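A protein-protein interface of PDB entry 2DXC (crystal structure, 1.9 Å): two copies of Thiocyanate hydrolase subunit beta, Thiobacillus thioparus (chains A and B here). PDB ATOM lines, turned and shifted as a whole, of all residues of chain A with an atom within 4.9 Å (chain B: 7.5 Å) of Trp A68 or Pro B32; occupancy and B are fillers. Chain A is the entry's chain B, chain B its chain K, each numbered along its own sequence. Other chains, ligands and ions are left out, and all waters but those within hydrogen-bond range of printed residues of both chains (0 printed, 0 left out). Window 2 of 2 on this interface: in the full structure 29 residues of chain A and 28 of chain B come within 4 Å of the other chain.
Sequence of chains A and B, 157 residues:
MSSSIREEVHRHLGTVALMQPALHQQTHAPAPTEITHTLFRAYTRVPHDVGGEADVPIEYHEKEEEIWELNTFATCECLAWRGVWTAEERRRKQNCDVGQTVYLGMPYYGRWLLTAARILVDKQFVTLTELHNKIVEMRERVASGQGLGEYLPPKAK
CB of Ala B31 touches CD of Lys A63 (3.97 Å).
CZ2 of Trp A68 touches CG of Pro B32, at 3.6 Å.
CG of Pro B32 touches OE2 of Glu A69, 3.7 Å away.
Pro A107 touches Pro B30 (CA to O, 3.2 Å).
Pro A107 touches Ala B31 (CG to C, 3.9 Å).
Pro B32 touches Pro A107.
Pro A107 touches Ile B35 (CG to CG1, 3.6 Å).
Of chain B, only Pro B32 comes within 4 Å of Trp A68.
Printed residues of chain A within 4 Å of Pro B32: Trp A68, Glu A69 and Pro A107.
Of the printed residues of chain B, Glu A69 touches Pro B32.
Printed residues of chain A within 4 Å of Pro B30: Pro A107 (3.2 Å).
Of the printed residues of chain B, Lys A63 touches Ala B31.
The nearest residue of chain B that does not touch Trp A68 is Thr B33 (7.0 Å).
The nearest residue of chain A that does not touch Pro B32 is Lys A63 (4.2 Å).
The nearest printed residue of chain B that does not touch Lys A63 is Pro B32 (4.2 Å).
NZ of Lys A63 is in salt-bridge range of OE1 of Glu A69 (2.9 Å).
N of Glu A66 sits at hydrogen-bond distance from OE1 of Glu A69.
The backbone carbonyl oxygen of Trp A68 lies within hydrogen-bond range of the side-chain hydroxyl of Thr A72 (2.7 Å).
No position is printed for both chains.
Of the 7 pairs that touch across the chains among the printed residues, none has its exchanged pair printed and touching as well.
Of the 13 printed residues of chain A, 4 touch a printed residue of chain B.
Hydrophobic or aromatic side chains of chain A within 4 Å of the printed part of chain B: Trp A68 and Pro A107.
Along chain A the printed residues that touch a printed residue of chain B span positions 63 to 107.
Among the printed residues, 7 pairs touch across the chains.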
ATOM      1  N   LYS A  63      14.113 -15.078  23.795  1.00  0.00           N
ATOM      2  CA  LYS A  63      14.676 -15.056  22.453  1.00  0.00           C
ATOM      3  C   LYS A  63      13.957 -14.005  21.626  1.00  0.00           C
ATOM      4  O   LYS A  63      12.724 -13.964  21.612  1.00  0.00           O
ATOM      5  CB  LYS A  63      14.543 -16.414  21.748  1.00  0.00           C
ATOM      6  CG  LYS A  63      15.300 -16.459  20.409  1.00  0.00           C
ATOM      7  CD  LYS A  63      15.043 -17.736  19.596  1.00  0.00           C
ATOM      8  CE  LYS A  63      13.735 -17.658  18.806  1.00  0.00           C
ATOM      9  NZ  LYS A  63      13.772 -16.603  17.735  1.00  0.00           N
ATOM     10  N   GLU A  66      12.082 -13.408  15.308  1.00  0.00           N
ATOM     11  CA  GLU A  66      12.587 -13.206  13.950  1.00  0.00           C
ATOM     12  C   GLU A  66      11.415 -12.665  13.139  1.00  0.00           C
ATOM     13  O   GLU A  66      10.258 -12.988  13.421  1.00  0.00           O
ATOM     14  CB  GLU A  66      13.043 -14.535  13.329  1.00  0.00           C
ATOM     15  CG  GLU A  66      14.218 -15.222  14.026  1.00  0.00           C
ATOM     16  CD  GLU A  66      15.565 -14.809  13.462  1.00  0.00           C
ATOM     17  OE1 GLU A  66      15.609 -13.917  12.588  1.00  0.00           O
ATOM     18  OE2 GLU A  66      16.587 -15.383  13.896  1.00  0.00           O
ATOM     19  N   ILE A  67      11.706 -11.839  12.142  1.00  0.00           N
ATOM     20  CA  ILE A  67      10.651 -11.303  11.302  1.00  0.00           C
ATOM     21  C   ILE A  67       9.884 -12.458  10.660  1.00  0.00           C
ATOM     22  O   ILE A  67       8.657 -12.422  10.577  1.00  0.00           O
ATOM     23  CB  ILE A  67      11.218 -10.406  10.180  1.00  0.00           C
ATOM     24  CG1 ILE A  67      11.835  -9.142  10.790  1.00  0.00           C
ATOM     25  CG2 ILE A  67      10.104 -10.035   9.199  1.00  0.00           C
ATOM     26  CD1 ILE A  67      12.562  -8.257   9.785  1.00  0.00           C
ATOM     27  N   TRP A  68      10.595 -13.491  10.220  1.00  0.00           N
ATOM     28  CA  TRP A  68       9.917 -14.609   9.581  1.00  0.00           C
ATOM     29  C   TRP A  68       9.044 -15.392  10.549  1.00  0.00           C
ATOM     30  O   TRP A  68       8.070 -16.021  10.135  1.00  0.00           O
ATOM     31  CB  TRP A  68      10.912 -15.548   8.878  1.00  0.00           C
ATOM     32  CG  TRP A  68      11.775 -16.404   9.759  1.00  0.00           C
ATOM     33  CD1 TRP A  68      13.049 -16.136  10.174  1.00  0.00           C
ATOM     34  CD2 TRP A  68      11.455 -17.708  10.270  1.00  0.00           C
ATOM     35  NE1 TRP A  68      13.543 -17.193  10.902  1.00  0.00           N
ATOM     36  CE2 TRP A  68      12.585 -18.169  10.977  1.00  0.00           C
ATOM     37  CE3 TRP A  68      10.321 -18.528  10.195  1.00  0.00           C
ATOM     38  CZ2 TRP A  68      12.620 -19.420  11.608  1.00  0.00           C
ATOM     39  CZ3 TRP A  68      10.354 -19.776  10.822  1.00  0.00           C
ATOM     40  CH2 TRP A  68      11.499 -20.206  11.519  1.00  0.00           C
ATOM     41  N   GLU A  69       9.380 -15.348  11.836  1.00  0.00           N
ATOM     42  CA  GLU A  69       8.581 -16.049  12.834  1.00  0.00           C
ATOM     43  C   GLU A  69       7.248 -15.320  12.998  1.00  0.00           C
ATOM     44  O   GLU A  69       6.196 -15.952  13.082  1.00  0.00           O
ATOM     45  CB  GLU A  69       9.322 -16.123  14.178  1.00  0.00           C
ATOM     46  CG  GLU A  69      10.604 -16.957  14.128  1.00  0.00           C
ATOM     47  CD  GLU A  69      11.302 -17.068  15.479  1.00  0.00           C
ATOM     48  OE1 GLU A  69      11.430 -16.036  16.171  1.00  0.00           O
ATOM     49  OE2 GLU A  69      11.738 -18.183  15.843  1.00  0.00           O
ATOM     50  N   LEU A  70       7.291 -13.992  13.039  1.00  0.00           N
ATOM     51  CA  LEU A  70       6.067 -13.209  13.170  1.00  0.00           C
ATOM     52  C   LEU A  70       5.194 -13.426  11.935  1.00  0.00           C
ATOM     53  O   LEU A  70       3.979 -13.566  12.042  1.00  0.00           O
ATOM     54  CB  LEU A  70       6.391 -11.719  13.328  1.00  0.00           C
ATOM     55  CG  LEU A  70       5.194 -10.758  13.310  1.00  0.00           C
ATOM     56  CD1 LEU A  70       4.064 -11.273  14.215  1.00  0.00           C
ATOM     57  CD2 LEU A  70       5.663  -9.376  13.764  1.00  0.00           C
ATOM     58  N   ASN A  71       5.820 -13.457  10.762  1.00  0.00           N
ATOM     59  CA  ASN A  71       5.089 -13.680   9.518  1.00  0.00           C
ATOM     60  C   ASN A  71       4.482 -15.086   9.469  1.00  0.00           C
ATOM     61  O   ASN A  71       3.365 -15.269   8.980  1.00  0.00           O
ATOM     62  CB  ASN A  71       6.019 -13.468   8.322  1.00  0.00           C
ATOM     63  CG  ASN A  71       6.277 -12.002   8.044  1.00  0.00           C
ATOM     64  OD1 ASN A  71       7.314 -11.631   7.489  1.00  0.00           O
ATOM     65  ND2 ASN A  71       5.324 -11.159   8.416  1.00  0.00           N
ATOM     66  N   THR A  72       5.214 -16.072   9.984  1.00  0.00           N
ATOM     67  CA  THR A  72       4.732 -17.453  10.000  1.00  0.00           C
ATOM     68  C   THR A  72       3.511 -17.584  10.908  1.00  0.00           C
ATOM     69  O   THR A  72       2.518 -18.222  10.545  1.00  0.00           O
ATOM     70  CB  THR A  72       5.833 -18.425  10.486  1.00  0.00           C
ATOM     71  OG1 THR A  72       6.921 -18.424   9.552  1.00  0.00           O
ATOM     72  CG2 THR A  72       5.280 -19.843  10.609  1.00  0.00           C
ATOM     73  N   PRO A 107      13.700 -26.059  14.852  1.00  0.00           N
ATOM     74  CA  PRO A 107      13.172 -25.002  15.724  1.00  0.00           C
ATOM     75  C   PRO A 107      11.644 -24.993  15.787  1.00  0.00           C
ATOM     76  O   PRO A 107      10.967 -25.439  14.862  1.00  0.00           O
ATOM     77  CB  PRO A 107      13.700 -23.713  15.082  1.00  0.00           C
ATOM     78  CG  PRO A 107      14.860 -24.170  14.238  1.00  0.00           C
ATOM     79  CD  PRO A 107      14.362 -25.473  13.677  1.00  0.00           C
ATOM     80  N   TYR A 109       9.288 -22.525  15.552  1.00  0.00           N
ATOM     81  CA  TYR A 109       8.648 -21.914  14.400  1.00  0.00           C
ATOM     82  C   TYR A 109       9.025 -22.556  13.074  1.00  0.00           C
ATOM     83  O   TYR A 109       8.349 -22.347  12.066  1.00  0.00           O
ATOM     84  CB  TYR A 109       8.919 -20.410  14.371  1.00  0.00           C
ATOM     85  CG  TYR A 109       7.837 -19.625  15.083  1.00  0.00           C
ATOM     86  CD1 TYR A 109       8.134 -18.806  16.171  1.00  0.00           C
ATOM     87  CD2 TYR A 109       6.502 -19.736  14.686  1.00  0.00           C
ATOM     88  CE1 TYR A 109       7.120 -18.115  16.850  1.00  0.00           C
ATOM     89  CE2 TYR A 109       5.484 -19.054  15.355  1.00  0.00           C
ATOM     90  CZ  TYR A 109       5.799 -18.248  16.433  1.00  0.00           C
ATOM     91  OH  TYR A 109       4.786 -17.580  17.087  1.00  0.00           O
ATOM     92  N   GLY A 110      10.095 -23.344  13.072  1.00  0.00           N
ATOM     93  CA  GLY A 110      10.485 -24.024  11.851  1.00  0.00           C
ATOM     94  C   GLY A 110       9.408 -25.053  11.550  1.00  0.00           C
ATOM     95  O   GLY A 110       9.049 -25.281  10.392  1.00  0.00           O
ATOM     96  N   LEU A 113       6.147 -23.320  10.287  1.00  0.00           N
ATOM     97  CA  LEU A 113       6.285 -22.945   8.884  1.00  0.00           C
ATOM     98  C   LEU A 113       6.218 -24.138   7.944  1.00  0.00           C
ATOM     99  O   LEU A 113       5.512 -24.100   6.940  1.00  0.00           O
ATOM    100  CB  LEU A 113       7.600 -22.190   8.666  1.00  0.00           C
ATOM    101  CG  LEU A 113       7.934 -21.850   7.210  1.00  0.00           C
ATOM    102  CD1 LEU A 113       6.793 -21.055   6.580  1.00  0.00           C
ATOM    103  CD2 LEU A 113       9.233 -21.060   7.162  1.00  0.00           C
ATOM    104  N   TYR A 151      12.939  -8.756   4.272  1.00  0.00           N
ATOM    105  CA  TYR A 151      14.091  -9.523   4.733  1.00  0.00           C
ATOM    106  C   TYR A 151      15.355  -8.994   4.067  1.00  0.00           C
ATOM    107  O   TYR A 151      16.404  -8.879   4.701  1.00  0.00           O
ATOM    108  CB  TYR A 151      13.941 -11.011   4.390  1.00  0.00           C
ATOM    109  CG  TYR A 151      12.727 -11.683   4.991  1.00  0.00           C
ATOM    110  CD1 TYR A 151      11.680 -12.126   4.184  1.00  0.00           C
ATOM    111  CD2 TYR A 151      12.623 -11.873   6.371  1.00  0.00           C
ATOM    112  CE1 TYR A 151      10.558 -12.742   4.734  1.00  0.00           C
ATOM    113  CE2 TYR A 151      11.503 -12.489   6.930  1.00  0.00           C
ATOM    114  CZ  TYR A 151      10.476 -12.920   6.105  1.00  0.00           C
ATOM    115  OH  TYR A 151       9.363 -13.522   6.648  1.00  0.00           O
ATOM    116  N   ALA B  29      14.877 -28.796  20.374  1.00  0.00           N
ATOM    117  CA  ALA B  29      14.266 -27.646  19.718  1.00  0.00           C
ATOM    118  C   ALA B  29      15.200 -26.430  19.685  1.00  0.00           C
ATOM    119  O   ALA B  29      14.887 -25.375  20.239  1.00  0.00           O
ATOM    120  CB  ALA B  29      12.945 -27.288  20.421  1.00  0.00           C
ATOM    121  N   PRO B  30      16.358 -26.562  19.024  1.00  0.00           N
ATOM    122  CA  PRO B  30      17.309 -25.447  18.942  1.00  0.00           C
ATOM    123  C   PRO B  30      16.746 -24.233  18.201  1.00  0.00           C
ATOM    124  O   PRO B  30      15.825 -24.356  17.393  1.00  0.00           O
ATOM    125  CB  PRO B  30      18.504 -26.067  18.220  1.00  0.00           C
ATOM    126  CG  PRO B  30      17.861 -27.108  17.347  1.00  0.00           C
ATOM    127  CD  PRO B  30      16.847 -27.731  18.272  1.00  0.00           C
ATOM    128  N   ALA B  31      17.303 -23.062  18.488  1.00  0.00           N
ATOM    129  CA  ALA B  31      16.872 -21.820  17.860  1.00  0.00           C
ATOM    130  C   ALA B  31      17.225 -21.839  16.373  1.00  0.00           C
ATOM    131  O   ALA B  31      18.137 -22.554  15.957  1.00  0.00           O
ATOM    132  CB  ALA B  31      17.546 -20.633  18.545  1.00  0.00           C
ATOM    133  N   PRO B  32      16.507 -21.053  15.554  1.00  0.00           N
ATOM    134  CA  PRO B  32      16.776 -21.006  14.112  1.00  0.00           C
ATOM    135  C   PRO B  32      18.233 -20.679  13.805  1.00  0.00           C
ATOM    136  O   PRO B  32      18.768 -21.089  12.776  1.00  0.00           O
ATOM    137  CB  PRO B  32      15.831 -19.914  13.623  1.00  0.00           C
ATOM    138  CG  PRO B  32      14.668 -20.059  14.548  1.00  0.00           C
ATOM    139  CD  PRO B  32      15.342 -20.215  15.890  1.00  0.00           C
ATOM    140  N   THR B  33      18.869 -19.940  14.704  1.00  0.00           N
ATOM    141  CA  THR B  33      20.261 -19.560  14.516  1.00  0.00           C
ATOM    142  C   THR B  33      21.226 -20.736  14.666  1.00  0.00           C
ATOM    143  O   THR B  33      22.417 -20.602  14.383  1.00  0.00           O
ATOM    144  CB  THR B  33      20.659 -18.427  15.493  1.00  0.00           C
ATOM    145  OG1 THR B  33      20.209 -18.743  16.817  1.00  0.00           O
ATOM    146  CG2 THR B  33      20.034 -17.112  15.052  1.00  0.00           C
ATOM    147  N   GLU B  34      20.714 -21.886  15.100  1.00  0.00           N
ATOM    148  CA  GLU B  34      21.550 -23.077  15.263  1.00  0.00           C
ATOM    149  C   GLU B  34      21.384 -24.022  14.083  1.00  0.00           C
ATOM    150  O   GLU B  34      22.007 -25.081  14.026  1.00  0.00           O
ATOM    151  CB  GLU B  34      21.195 -23.817  16.556  1.00  0.00           C
ATOM    152  CG  GLU B  34      21.502 -23.029  17.814  1.00  0.00           C
ATOM    153  CD  GLU B  34      22.914 -22.486  17.812  1.00  0.00           C
ATOM    154  OE1 GLU B  34      23.866 -23.295  17.787  1.00  0.00           O
ATOM    155  OE2 GLU B  34      23.072 -21.247  17.828  1.00  0.00           O
ATOM    156  N   ILE B  35      20.539 -23.636  13.137  1.00  0.00           N
ATOM    157  CA  ILE B  35      20.291 -24.467  11.970  1.00  0.00           C
ATOM    158  C   ILE B  35      21.001 -23.899  10.753  1.00  0.00           C
ATOM    159  O   ILE B  35      20.670 -22.812  10.289  1.00  0.00           O
ATOM    160  CB  ILE B  35      18.783 -24.556  11.659  1.00  0.00           C
ATOM    161  CG1 ILE B  35      18.035 -25.081  12.884  1.00  0.00           C
ATOM    162  CG2 ILE B  35      18.545 -25.484  10.472  1.00  0.00           C
ATOM    163  CD1 ILE B  35      18.426 -26.511  13.305  1.00  0.00           C
ATOM    164  N   THR B  36      21.981 -24.639  10.248  1.00  0.00           N
ATOM    165  CA  THR B  36      22.722 -24.227   9.064  1.00  0.00           C
ATOM    166  C   THR B  36      21.954 -24.773   7.866  1.00  0.00           C
ATOM    167  O   THR B  36      21.049 -25.590   8.034  1.00  0.00           O
ATOM    168  CB  THR B  36      24.122 -24.850   9.040  1.00  0.00           C
ATOM    169  OG1 THR B  36      24.000 -26.275   9.090  1.00  0.00           O
ATOM    170  CG2 THR B  36      24.945 -24.372  10.232  1.00  0.00           C
